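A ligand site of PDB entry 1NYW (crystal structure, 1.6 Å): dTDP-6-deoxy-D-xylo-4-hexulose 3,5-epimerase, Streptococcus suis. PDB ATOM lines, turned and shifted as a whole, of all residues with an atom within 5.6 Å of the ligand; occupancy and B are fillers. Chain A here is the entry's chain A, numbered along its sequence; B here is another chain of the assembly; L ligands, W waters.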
ATOM      1  N   GLN A  61     -24.971   8.544  13.287  1.00  0.00           N
ATOM      2  CA  GLN A  61     -24.167   8.902  12.122  1.00  0.00           C
ATOM      3  C   GLN A  61     -24.623  10.294  11.671  1.00  0.00           C
ATOM      4  O   GLN A  61     -25.763  10.607  11.767  1.00  0.00           O
ATOM      5  CB  GLN A  61     -24.397   7.895  11.010  1.00  0.00           C
ATOM      6  CG  GLN A  61     -23.838   8.248   9.653  1.00  0.00           C
ATOM      7  CD  GLN A  61     -23.971   7.171   8.572  1.00  0.00           C
ATOM      8  OE1 GLN A  61     -24.358   6.037   8.859  1.00  0.00           O
ATOM      9  NE2 GLN A  61     -23.686   7.437   7.372  1.00  0.00           N
ATOM     10  N   ASN A  63     -24.251  12.800   8.424  1.00  0.00           N
ATOM     11  CA  ASN A  63     -23.858  12.944   7.044  1.00  0.00           C
ATOM     12  C   ASN A  63     -23.978  14.409   6.630  1.00  0.00           C
ATOM     13  O   ASN A  63     -24.824  15.162   7.142  1.00  0.00           O
ATOM     14  CB  ASN A  63     -24.757  12.117   6.112  1.00  0.00           C
ATOM     15  CG  ASN A  63     -24.695  10.599   6.331  1.00  0.00           C
ATOM     16  OD1 ASN A  63     -25.665   9.871   6.114  1.00  0.00           O
ATOM     17  ND2 ASN A  63     -23.560  10.111   6.789  1.00  0.00           N
ATOM     18  N   SER A  65     -23.852  16.790   2.940  1.00  0.00           N
ATOM     19  CA  SER A  65     -23.676  16.967   1.491  1.00  0.00           C
ATOM     20  C   SER A  65     -23.525  18.451   1.213  1.00  0.00           C
ATOM     21  O   SER A  65     -24.035  19.342   1.891  1.00  0.00           O
ATOM     22  CB  SER A  65     -24.828  16.376   0.617  1.00  0.00           C
ATOM     23  OG  SER A  65     -26.056  16.919   0.982  1.00  0.00           O
ATOM     24  N   ARG A  73     -31.916  16.135  -4.979  1.00  0.00           N
ATOM     25  CA  ARG A  73     -31.498  14.851  -4.427  1.00  0.00           C
ATOM     26  C   ARG A  73     -32.768  14.237  -3.830  1.00  0.00           C
ATOM     27  O   ARG A  73     -33.387  14.875  -3.006  1.00  0.00           O
ATOM     28  CB  ARG A  73     -30.405  14.928  -3.338  1.00  0.00           C
ATOM     29  CG  ARG A  73     -29.239  15.726  -3.768  1.00  0.00           C
ATOM     30  CD  ARG A  73     -28.017  15.421  -2.802  1.00  0.00           C
ATOM     31  NE  ARG A  73     -26.891  16.267  -3.089  1.00  0.00           N
ATOM     32  CZ  ARG A  73     -25.645  15.781  -3.175  1.00  0.00           C
ATOM     33  NH1 ARG A  73     -25.401  14.501  -2.988  1.00  0.00           N
ATOM     34  NH2 ARG A  73     -24.613  16.613  -3.470  1.00  0.00           N
ATOM     35  N   GLY A  74     -33.109  13.031  -4.236  1.00  0.00           N
ATOM     36  CA  GLY A  74     -34.291  12.360  -3.702  1.00  0.00           C
ATOM     37  C   GLY A  74     -34.966  11.485  -4.757  1.00  0.00           C
ATOM     38  O   GLY A  74     -34.467  11.396  -5.891  1.00  0.00           O
ATOM     39  N   HIS A  76     -35.774   9.569  -1.170  1.00  0.00           N
ATOM     40  CA  HIS A  76     -35.127   8.452  -0.526  1.00  0.00           C
ATOM     41  C   HIS A  76     -35.785   8.143   0.817  1.00  0.00           C
ATOM     42  O   HIS A  76     -35.778   9.015   1.683  1.00  0.00           O
ATOM     43  CB  HIS A  76     -33.669   8.803  -0.297  1.00  0.00           C
ATOM     44  CG  HIS A  76     -32.964   9.275  -1.547  1.00  0.00           C
ATOM     45  ND1 HIS A  76     -32.068  10.323  -1.546  1.00  0.00           N
ATOM     46  CD2 HIS A  76     -33.013   8.834  -2.823  1.00  0.00           C
ATOM     47  CE1 HIS A  76     -31.583  10.490  -2.768  1.00  0.00           C
ATOM     48  NE2 HIS A  76     -32.139   9.597  -3.557  1.00  0.00           N
ATOM     49  N   GLU A  78     -34.995   5.429   3.252  1.00  0.00           N
ATOM     50  CA  GLU A  78     -34.232   4.353   3.899  1.00  0.00           C
ATOM     51  C   GLU A  78     -34.796   4.018   5.283  1.00  0.00           C
ATOM     52  O   GLU A  78     -35.439   4.850   5.905  1.00  0.00           O
ATOM     53  CB  GLU A  78     -32.765   4.739   4.002  1.00  0.00           C
ATOM     54  CG  GLU A  78     -32.076   4.979   2.640  1.00  0.00           C
ATOM     55  CD  GLU A  78     -31.826   6.428   2.382  1.00  0.00           C
ATOM     56  OE1 GLU A  78     -32.771   7.190   2.633  1.00  0.00           O
ATOM     57  OE2 GLU A  78     -30.704   6.782   1.965  1.00  0.00           O
ATOM     58  N   TRP A  80     -34.355   4.213   8.438  1.00  0.00           N
ATOM     59  CA  TRP A  80     -33.887   4.880   9.639  1.00  0.00           C
ATOM     60  C   TRP A  80     -34.494   6.278   9.715  1.00  0.00           C
ATOM     61  O   TRP A  80     -34.929   6.821   8.699  1.00  0.00           O
ATOM     62  CB  TRP A  80     -32.355   4.942   9.708  1.00  0.00           C
ATOM     63  CG  TRP A  80     -31.690   5.412   8.470  1.00  0.00           C
ATOM     64  CD1 TRP A  80     -31.568   6.702   8.022  1.00  0.00           C
ATOM     65  CD2 TRP A  80     -30.992   4.589   7.518  1.00  0.00           C
ATOM     66  NE1 TRP A  80     -30.851   6.724   6.842  1.00  0.00           N
ATOM     67  CE2 TRP A  80     -30.515   5.430   6.511  1.00  0.00           C
ATOM     68  CE3 TRP A  80     -30.794   3.221   7.376  1.00  0.00           C
ATOM     69  CZ2 TRP A  80     -29.830   4.949   5.414  1.00  0.00           C
ATOM     70  CZ3 TRP A  80     -30.077   2.732   6.297  1.00  0.00           C
ATOM     71  CH2 TRP A  80     -29.647   3.587   5.316  1.00  0.00           C
ATOM     72  N   LYS A  82     -34.318  10.412  10.386  1.00  0.00           N
ATOM     73  CA  LYS A  82     -33.401  11.482  10.018  1.00  0.00           C
ATOM     74  C   LYS A  82     -33.805  12.780  10.715  1.00  0.00           C
ATOM     75  O   LYS A  82     -34.955  13.121  10.796  1.00  0.00           O
ATOM     76  CB  LYS A  82     -33.448  11.709   8.512  1.00  0.00           C
ATOM     77  CG  LYS A  82     -33.123  10.502   7.659  1.00  0.00           C
ATOM     78  CD  LYS A  82     -33.354  10.790   6.171  1.00  0.00           C
ATOM     79  CE  LYS A  82     -33.021   9.574   5.310  1.00  0.00           C
ATOM     80  NZ  LYS A  82     -33.625   9.576   3.910  1.00  0.00           N
ATOM     81  N   ILE A  84     -32.778  16.612   9.899  1.00  0.00           N
ATOM     82  CA  ILE A  84     -32.196  17.343   8.761  1.00  0.00           C
ATOM     83  C   ILE A  84     -32.152  18.841   9.039  1.00  0.00           C
ATOM     84  O   ILE A  84     -33.083  19.406   9.594  1.00  0.00           O
ATOM     85  CB  ILE A  84     -33.023  17.062   7.524  1.00  0.00           C
ATOM     86  CG1 ILE A  84     -32.893  15.602   7.141  1.00  0.00           C
ATOM     87  CG2 ILE A  84     -32.586  17.989   6.356  1.00  0.00           C
ATOM     88  CD1 ILE A  84     -34.072  15.157   6.336  1.00  0.00           C
ATOM     89  N   ASN A 127     -37.397  11.418   1.565  1.00  0.00           N
ATOM     90  CA  ASN A 127     -36.792  12.718   1.807  1.00  0.00           C
ATOM     91  C   ASN A 127     -36.177  13.157   0.507  1.00  0.00           C
ATOM     92  O   ASN A 127     -35.467  12.381  -0.200  1.00  0.00           O
ATOM     93  CB  ASN A 127     -35.658  12.557   2.842  1.00  0.00           C
ATOM     94  CG  ASN A 127     -35.017  13.834   3.232  1.00  0.00           C
ATOM     95  OD1 ASN A 127     -35.642  14.754   3.757  1.00  0.00           O
ATOM     96  ND2 ASN A 127     -33.717  13.923   3.019  1.00  0.00           N
ATOM     97  N   GLY A 128     -36.331  14.427   0.231  1.00  0.00           N
ATOM     98  CA  GLY A 128     -35.678  15.033  -0.883  1.00  0.00           C
ATOM     99  C   GLY A 128     -35.493  16.509  -0.677  1.00  0.00           C
ATOM    100  O   GLY A 128     -35.934  17.125   0.227  1.00  0.00           O
ATOM    101  N   PHE A 129     -34.717  17.124  -1.607  1.00  0.00           N
ATOM    102  CA  PHE A 129     -34.608  18.592  -1.613  1.00  0.00           C
ATOM    103  C   PHE A 129     -34.064  19.070  -2.944  1.00  0.00           C
ATOM    104  O   PHE A 129     -33.447  18.313  -3.684  1.00  0.00           O
ATOM    105  CB  PHE A 129     -33.675  19.150  -0.501  1.00  0.00           C
ATOM    106  CG  PHE A 129     -32.253  18.745  -0.617  1.00  0.00           C
ATOM    107  CD1 PHE A 129     -31.319  19.557  -1.313  1.00  0.00           C
ATOM    108  CD2 PHE A 129     -31.821  17.589  -0.050  1.00  0.00           C
ATOM    109  CE1 PHE A 129     -29.940  19.207  -1.421  1.00  0.00           C
ATOM    110  CE2 PHE A 129     -30.422  17.218  -0.137  1.00  0.00           C
ATOM    111  CZ  PHE A 129     -29.507  18.026  -0.823  1.00  0.00           C
ATOM    112  N   TYR A 138     -25.878  20.671   3.601  1.00  0.00           N
ATOM    113  CA  TYR A 138     -27.008  19.944   4.192  1.00  0.00           C
ATOM    114  C   TYR A 138     -26.423  18.928   5.177  1.00  0.00           C
ATOM    115  O   TYR A 138     -25.672  18.049   4.747  1.00  0.00           O
ATOM    116  CB  TYR A 138     -27.811  19.307   3.050  1.00  0.00           C
ATOM    117  CG  TYR A 138     -29.061  18.582   3.298  1.00  0.00           C
ATOM    118  CD1 TYR A 138     -30.282  19.222   3.108  1.00  0.00           C
ATOM    119  CD2 TYR A 138     -29.044  17.269   3.645  1.00  0.00           C
ATOM    120  CE1 TYR A 138     -31.466  18.545   3.263  1.00  0.00           C
ATOM    121  CE2 TYR A 138     -30.260  16.536   3.846  1.00  0.00           C
ATOM    122  CZ  TYR A 138     -31.432  17.202   3.612  1.00  0.00           C
ATOM    123  OH  TYR A 138     -32.682  16.575   3.771  1.00  0.00           O
ATOM    124  N   TYR A 140     -27.225  16.154   8.438  1.00  0.00           N
ATOM    125  CA  TYR A 140     -28.330  15.442   9.053  1.00  0.00           C
ATOM    126  C   TYR A 140     -27.797  14.339   9.932  1.00  0.00           C
ATOM    127  O   TYR A 140     -26.727  13.808   9.672  1.00  0.00           O
ATOM    128  CB  TYR A 140     -29.400  14.934   8.025  1.00  0.00           C
ATOM    129  CG  TYR A 140     -29.003  13.885   7.040  1.00  0.00           C
ATOM    130  CD1 TYR A 140     -29.537  12.608   7.138  1.00  0.00           C
ATOM    131  CD2 TYR A 140     -28.115  14.167   5.965  1.00  0.00           C
ATOM    132  CE1 TYR A 140     -29.124  11.616   6.238  1.00  0.00           C
ATOM    133  CE2 TYR A 140     -27.734  13.170   5.062  1.00  0.00           C
ATOM    134  CZ  TYR A 140     -28.253  11.897   5.201  1.00  0.00           C
ATOM    135  OH  TYR A 140     -27.945  10.878   4.295  1.00  0.00           O
ATOM    136  N   TRP A 146     -26.016   2.961   6.837  1.00  0.00           N
ATOM    137  CA  TRP A 146     -26.165   2.699   5.414  1.00  0.00           C
ATOM    138  C   TRP A 146     -24.993   1.861   4.913  1.00  0.00           C
ATOM    139  O   TRP A 146     -23.862   1.977   5.413  1.00  0.00           O
ATOM    140  CB  TRP A 146     -26.202   4.037   4.687  1.00  0.00           C
ATOM    141  CG  TRP A 146     -26.338   4.119   3.157  1.00  0.00           C
ATOM    142  CD1 TRP A 146     -27.489   4.358   2.432  1.00  0.00           C
ATOM    143  CD2 TRP A 146     -25.270   4.075   2.184  1.00  0.00           C
ATOM    144  NE1 TRP A 146     -27.200   4.423   1.094  1.00  0.00           N
ATOM    145  CE2 TRP A 146     -25.850   4.281   0.911  1.00  0.00           C
ATOM    146  CE3 TRP A 146     -23.893   3.895   2.266  1.00  0.00           C
ATOM    147  CZ2 TRP A 146     -25.122   4.296  -0.261  1.00  0.00           C
ATOM    148  CZ3 TRP A 146     -23.133   3.961   1.070  1.00  0.00           C
ATOM    149  CH2 TRP A 146     -23.773   4.134  -0.177  1.00  0.00           C
ATOM    150  N   LEU A 148     -23.836   0.493   0.765  1.00  0.00           N
ATOM    151  CA  LEU A 148     -24.158   0.504  -0.649  1.00  0.00           C
ATOM    152  C   LEU A 148     -24.667  -0.827  -1.165  1.00  0.00           C
ATOM    153  O   LEU A 148     -25.599  -0.863  -1.941  1.00  0.00           O
ATOM    154  CB  LEU A 148     -22.957   0.919  -1.483  1.00  0.00           C
ATOM    155  CG  LEU A 148     -23.125   1.919  -2.612  1.00  0.00           C
ATOM    156  CD1 LEU A 148     -22.012   1.814  -3.584  1.00  0.00           C
ATOM    157  CD2 LEU A 148     -24.443   1.850  -3.286  1.00  0.00           C
ATOM    158  N   LYS A 151     -28.286  -1.092  -0.547  1.00  0.00           N
ATOM    159  CA  LYS A 151     -29.128  -0.087  -1.199  1.00  0.00           C
ATOM    160  C   LYS A 151     -30.337  -0.655  -1.974  1.00  0.00           C
ATOM    161  O   LYS A 151     -31.401  -0.066  -1.900  1.00  0.00           O
ATOM    162  CB  LYS A 151     -28.292   0.782  -2.103  1.00  0.00           C
ATOM    163  CG  LYS A 151     -29.089   1.907  -2.736  1.00  0.00           C
ATOM    164  CD  LYS A 151     -28.201   3.008  -3.297  1.00  0.00           C
ATOM    165  CE  LYS A 151     -29.087   4.118  -3.811  1.00  0.00           C
ATOM    166  NZ  LYS A 151     -28.356   5.034  -4.699  1.00  0.00           N
ATOM    167  N   PHE A 156     -37.354   3.968  -2.634  1.00  0.00           N
ATOM    168  CA  PHE A 156     -37.084   5.182  -3.394  1.00  0.00           C
ATOM    169  C   PHE A 156     -38.268   5.417  -4.315  1.00  0.00           C
ATOM    170  O   PHE A 156     -38.922   4.451  -4.748  1.00  0.00           O
ATOM    171  CB  PHE A 156     -35.836   5.004  -4.262  1.00  0.00           C
ATOM    172  CG  PHE A 156     -34.610   4.602  -3.530  1.00  0.00           C
ATOM    173  CD1 PHE A 156     -34.122   3.303  -3.586  1.00  0.00           C
ATOM    174  CD2 PHE A 156     -33.921   5.550  -2.777  1.00  0.00           C
ATOM    175  CE1 PHE A 156     -32.974   2.974  -2.895  1.00  0.00           C
ATOM    176  CE2 PHE A 156     -32.785   5.234  -2.114  1.00  0.00           C
ATOM    177  CZ  PHE A 156     -32.303   3.965  -2.158  1.00  0.00           C
ATOM    178  N   SER A 177     -28.481  12.736  -9.771  1.00  0.00           N
ATOM    179  CA  SER A 177     -27.631  11.567  -9.963  1.00  0.00           C
ATOM    180  C   SER A 177     -28.229  10.534 -10.905  1.00  0.00           C
ATOM    181  O   SER A 177     -29.444  10.554 -11.200  1.00  0.00           O
ATOM    182  CB  SER A 177     -27.351  10.917  -8.618  1.00  0.00           C
ATOM    183  OG  SER A 177     -28.537  10.323  -8.098  1.00  0.00           O
ATOM    184  N   ALA A 179     -28.534   7.499 -10.236  1.00  0.00           N
ATOM    185  CA  ALA A 179     -29.411   6.697  -9.405  1.00  0.00           C
ATOM    186  C   ALA A 179     -30.769   7.338  -9.291  1.00  0.00           C
ATOM    187  O   ALA A 179     -31.796   6.651  -9.433  1.00  0.00           O
ATOM    188  CB  ALA A 179     -28.808   6.506  -8.029  1.00  0.00           C
ATOM    189  N   ASP A 180     -30.796   8.659  -9.116  1.00  0.00           N
ATOM    190  CA  ASP A 180     -32.069   9.345  -8.917  1.00  0.00           C
ATOM    191  C   ASP A 180     -32.885   9.435 -10.213  1.00  0.00           C
ATOM    192  O   ASP A 180     -34.112   9.445 -10.155  1.00  0.00           O
ATOM    193  CB  ASP A 180     -31.887  10.711  -8.285  1.00  0.00           C
ATOM    194  CG  ASP A 180     -31.642  10.645  -6.784  1.00  0.00           C
ATOM    195  OD1 ASP A 180     -31.816   9.561  -6.192  1.00  0.00           O
ATOM    196  OD2 ASP A 180     -31.230  11.625  -6.100  1.00  0.00           O
ATOM    197  N   HIS B  29     -16.911  12.062  -1.056  1.00  0.00           N
ATOM    198  CA  HIS B  29     -17.230  11.525  -2.388  1.00  0.00           C
ATOM    199  C   HIS B  29     -17.789  12.592  -3.282  1.00  0.00           C
ATOM    200  O   HIS B  29     -18.772  13.175  -2.930  1.00  0.00           O
ATOM    201  CB  HIS B  29     -18.248  10.410  -2.247  1.00  0.00           C
ATOM    202  CG  HIS B  29     -17.835   9.375  -1.245  1.00  0.00           C
ATOM    203  ND1 HIS B  29     -18.414   9.248  -0.001  1.00  0.00           N
ATOM    204  CD2 HIS B  29     -16.867   8.431  -1.309  1.00  0.00           C
ATOM    205  CE1 HIS B  29     -17.791   8.278   0.660  1.00  0.00           C
ATOM    206  NE2 HIS B  29     -16.871   7.754  -0.119  1.00  0.00           N
ATOM    207  N   ASP B  31     -19.302  14.117  -7.000  1.00  0.00           N
ATOM    208  CA  ASP B  31     -20.004  13.795  -8.249  1.00  0.00           C
ATOM    209  C   ASP B  31     -20.505  15.088  -8.921  1.00  0.00           C
ATOM    210  O   ASP B  31     -20.096  16.179  -8.534  1.00  0.00           O
ATOM    211  CB  ASP B  31     -21.122  12.738  -8.058  1.00  0.00           C
ATOM    212  CG  ASP B  31     -22.303  13.226  -7.235  1.00  0.00           C
ATOM    213  OD1 ASP B  31     -22.381  14.430  -6.870  1.00  0.00           O
ATOM    214  OD2 ASP B  31     -23.212  12.419  -6.937  1.00  0.00           O
ATOM    215  N   ARG B  33     -23.112  16.636  -8.598  1.00  0.00           N
ATOM    216  CA  ARG B  33     -23.905  17.514  -7.740  1.00  0.00           C
ATOM    217  C   ARG B  33     -23.089  18.284  -6.685  1.00  0.00           C
ATOM    218  O   ARG B  33     -23.572  19.279  -6.142  1.00  0.00           O
ATOM    219  CB  ARG B  33     -25.008  16.726  -7.033  1.00  0.00           C
ATOM    220  CG  ARG B  33     -25.860  15.860  -7.959  1.00  0.00           C
ATOM    221  CD  ARG B  33     -26.741  14.859  -7.251  1.00  0.00           C
ATOM    222  NE  ARG B  33     -25.882  13.818  -6.591  1.00  0.00           N
ATOM    223  CZ  ARG B  33     -26.312  12.901  -5.725  1.00  0.00           C
ATOM    224  NH1 ARG B  33     -27.625  12.854  -5.400  1.00  0.00           N
ATOM    225  NH2 ARG B  33     -25.470  11.992  -5.241  1.00  0.00           N
ATOM    226  N   PHE B  36     -20.480  14.359  -0.879  1.00  0.00           N
ATOM    227  CA  PHE B  36     -21.118  13.756   0.276  1.00  0.00           C
ATOM    228  C   PHE B  36     -20.089  13.171   1.135  1.00  0.00           C
ATOM    229  O   PHE B  36     -19.176  12.576   0.622  1.00  0.00           O
ATOM    230  CB  PHE B  36     -22.086  12.674  -0.229  1.00  0.00           C
ATOM    231  CG  PHE B  36     -22.899  12.022   0.851  1.00  0.00           C
ATOM    232  CD1 PHE B  36     -24.219  12.321   1.072  1.00  0.00           C
ATOM    233  CD2 PHE B  36     -22.280  11.066   1.641  1.00  0.00           C
ATOM    234  CE1 PHE B  36     -24.921  11.719   2.113  1.00  0.00           C
ATOM    235  CE2 PHE B  36     -22.961  10.427   2.625  1.00  0.00           C
ATOM    236  CZ  PHE B  36     -24.285  10.759   2.872  1.00  0.00           C
ATOM    237  N   GLU B  38     -19.749  10.952   5.124  1.00  0.00           N
ATOM    238  CA  GLU B  38     -20.198  10.496   6.470  1.00  0.00           C
ATOM    239  C   GLU B  38     -19.304  11.215   7.456  1.00  0.00           C
ATOM    240  O   GLU B  38     -18.216  10.826   7.674  1.00  0.00           O
ATOM    241  CB  GLU B  38     -20.104   9.010   6.675  1.00  0.00           C
ATOM    242  CG  GLU B  38     -20.764   8.171   5.635  1.00  0.00           C
ATOM    243  CD  GLU B  38     -20.668   6.674   5.869  1.00  0.00           C
ATOM    244  OE1 GLU B  38     -19.845   6.182   6.695  1.00  0.00           O
ATOM    245  OE2 GLU B  38     -21.419   5.919   5.198  1.00  0.00           O
ATOM    246  N   LYS B  44     -18.125   2.738  12.444  1.00  0.00           N
ATOM    247  CA  LYS B  44     -16.833   2.703  11.742  1.00  0.00           C
ATOM    248  C   LYS B  44     -15.696   3.421  12.462  1.00  0.00           C
ATOM    249  O   LYS B  44     -14.548   3.161  12.202  1.00  0.00           O
ATOM    250  CB  LYS B  44     -16.958   3.381  10.389  1.00  0.00           C
ATOM    251  CG  LYS B  44     -17.761   2.607   9.369  1.00  0.00           C
ATOM    252  CD  LYS B  44     -17.939   3.384   8.084  1.00  0.00           C
ATOM    253  CE  LYS B  44     -18.983   2.688   7.186  1.00  0.00           C
ATOM    254  NZ  LYS B  44     -19.139   3.382   5.821  1.00  0.00           N
HETATM  255  O1  LIG L   1     -27.533  14.672   0.510  1.00  0.00           O
HETATM  256  C1  LIG L   1     -28.533  14.236   1.450  1.00  0.00           C
HETATM  257  C2  LIG L   1     -29.121  12.901   1.037  1.00  0.00           C
HETATM  258  O2  LIG L   1     -28.038  11.999   1.055  1.00  0.00           O
HETATM  259  C3  LIG L   1     -30.179  12.378   1.985  1.00  0.00           C
HETATM  260  O3  LIG L   1     -31.192  13.413   1.932  1.00  0.00           O
HETATM  261  C4  LIG L   1     -30.520  10.926   1.546  1.00  0.00           C
HETATM  262  O4  LIG L   1     -31.320  10.219   2.530  1.00  0.00           O
HETATM  263  C5  LIG L   1     -29.281  10.027   1.330  1.00  0.00           C
HETATM  264  O5  LIG L   1     -29.544   8.793   0.666  1.00  0.00           O
HETATM  265  C6  LIG L   1     -28.252  10.743   0.488  1.00  0.00           C
HETATM  266  O6  LIG L   1     -28.662  10.812  -0.864  1.00  0.00           O
HETATM  267  P1  LIG L   1     -27.715  11.439  -1.994  1.00  0.00           P
HETATM  268  O7  LIG L   1     -28.503  11.365  -3.335  1.00  0.00           O
HETATM  269  O8  LIG L   1     -27.215  12.844  -1.535  1.00  0.00           O
HETATM  270  O9  LIG L   1     -26.514  10.407  -1.893  1.00  0.00           O
HETATM  271  P2  LIG L   1     -26.129   9.113  -2.767  1.00  0.00           P
HETATM  272  O10 LIG L   1     -26.991   7.887  -2.218  1.00  0.00           O
HETATM  273  O11 LIG L   1     -26.108   9.526  -4.277  1.00  0.00           O
HETATM  274  O12 LIG L   1     -24.629   8.917  -2.211  1.00  0.00           O
HETATM  275  C7  LIG L   1     -23.613   9.841  -2.470  1.00  0.00           C
HETATM  276  C8  LIG L   1     -22.223   9.242  -2.162  1.00  0.00           C
HETATM  277  O13 LIG L   1     -22.122   9.037  -0.744  1.00  0.00           O
HETATM  278  C9  LIG L   1     -22.050   7.899  -2.812  1.00  0.00           C
HETATM  279  O14 LIG L   1     -20.695   7.778  -3.326  1.00  0.00           O
HETATM  280  C10 LIG L   1     -22.332   6.886  -1.719  1.00  0.00           C
HETATM  281  C11 LIG L   1     -21.929   7.650  -0.462  1.00  0.00           C
HETATM  282  N1  LIG L   1     -22.724   7.412   0.763  1.00  0.00           N
HETATM  283  C12 LIG L   1     -24.052   7.688   0.758  1.00  0.00           C
HETATM  284  C13 LIG L   1     -24.751   7.531   1.955  1.00  0.00           C
HETATM  285  C14 LIG L   1     -26.266   7.780   2.011  1.00  0.00           C
HETATM  286  C15 LIG L   1     -22.094   7.063   1.892  1.00  0.00           C
HETATM  287  O15 LIG L   1     -20.807   6.851   1.925  1.00  0.00           O
HETATM  288  N2  LIG L   1     -22.734   6.919   3.060  1.00  0.00           N
HETATM  289  C16 LIG L   1     -24.044   7.140   3.086  1.00  0.00           C
HETATM  290  O16 LIG L   1     -24.613   6.971   4.283  1.00  0.00           O
HETATM  291  O   HOH W   1     -29.379   8.553   4.714  1.00  0.00           O
HETATM  292  O   HOH W   2     -32.598  13.143  -0.480  1.00  0.00           O
HETATM  293  O   HOH W   3     -26.050   5.562  -3.319  1.00  0.00           O
HETATM  294  O   HOH W   4     -29.627   5.460  -0.180  1.00  0.00           O
HETATM  295  O   HOH W   5     -29.493   7.408  -1.990  1.00  0.00           O
HETATM  296  O   HOH W   6     -27.046   7.350   5.493  1.00  0.00           O
HETATM  297  O   HOH W   7     -28.642   9.544  -5.489  1.00  0.00           O
HETATM  298  O   HOH W   8     -20.519   9.852  -5.332  1.00  0.00           O
HETATM  299  O   HOH W   9     -19.381   5.085   0.581  1.00  0.00           O
HETATM  300  O   HOH W  10     -18.123   7.028   3.214  1.00  0.00           O
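Asn 63 touches the ligand.
His 76 touches the ligand (CE1 to O7, 3.3 Å).
CE2 of Phe 129 touches C1 of the ligand (3.9 Å).
Tyr 138 touches the ligand (CE2 to C1, 3.7 Å).
CE3 of Trp 146 touches N2 of the ligand, at 3.3 Å.
Asp 180 touches the ligand (OD2 to O7, 3.9 Å).
His 29 of chain B touches the ligand (CE1 to O15, 3.6 Å).
Phe 36 of chain B touches the ligand.
Water W3 lies within hydrogen-bond range of the side-chain amino group of Lys 151 and an oxygen (O10) of the ligand.
Water W6 lies within hydrogen-bond range of O16 of the ligand (2.7 Å) and OD1 of Asn 63 (2.9 Å).
Water W2 lies within hydrogen-bond range of an oxygen (O3) of the ligand (2.8 Å), the backbone carbonyl oxygen of Asn 127 (3.0 Å), a ring nitrogen (ND1) of His 76 (3.1 Å) and the backbone carbonyl oxygen of Arg 73 (3.2 Å).
Water W7 lies within hydrogen-bond range of OG of Ser 177 (2.7 Å), O11 of the ligand (2.8 Å), OD1 of Asp 180 (3.3 Å) and NH1 of Arg 33 of chain B (3.5 Å).
Water W1 lies within hydrogen-bond range of the side-chain hydroxyl of Tyr 140, the indole nitrogen of Trp 80 and an oxygen (O4) of the ligand.
Water W4 lies within hydrogen-bond range of OE2 of Glu 78 (2.7 Å), NE1 of Trp 146 (2.9 Å) and O5 of the ligand (3.4 Å).
OE2 of Glu 78 lies within hydrogen-bond range of O5 of the ligand.
The guanidinium group (NH1) of Arg 33 of chain B is in salt-bridge range of an oxygen (O7) of the ligand (2.7 Å).
OE2 of Glu 38 of chain B is in hydrogen-bond range of N2 of the ligand (2.7 Å).
OG of Ser 65 sits at hydrogen-bond distance from O1 of the ligand (2.7 Å).
An oxygen (O4) of the ligand sits at hydrogen-bond distance from the side-chain amino group (NZ) of Lys 82 (2.8 Å).
ND2 of Asn 127 is in hydrogen-bond range of O3 of the ligand (2.8 Å).
NH1 of Arg 73 is in salt-bridge range of O8 of the ligand (2.9 Å).
The side-chain amide nitrogen (NE2) of Gln 61 sits at hydrogen-bond distance from an oxygen (O16) of the ligand, 3.3 Å away.
O2 of the ligand lies close to OH of Tyr 140, 3.4 Å away.
OD2 of Asp 180 is in salt-bridge range of NH1 of Arg 33 of chain B (3.9 Å).
The guanidinium group (NH2) of Arg 33 of chain B is in salt-bridge range of the side-chain carboxylate (OD2) of Asp 31 of chain B, 2.9 Å away.
The backbone carbonyl oxygen (O) of Ser 65 is in hydrogen-bond range of the backbone NH (N) of Tyr 138, at 2.8 Å.
The side-chain amide nitrogen (ND2) of Asn 127 lies within hydrogen-bond range of the side-chain hydroxyl (OH) of Tyr 138.
OD1 of Asp 180 sits at hydrogen-bond distance from NE2 of His 76 (2.7 Å).
NE2 of Gln 61 sits close to ND2 of Asn 63 (2.7 Å).
O of Asn 63 sits at hydrogen-bond distance from N of Tyr 140, 2.9 Å away.
The backbone NH of Asp 180 is in hydrogen-bond range of the side-chain hydroxyl of Ser 177, at 3.0 Å.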
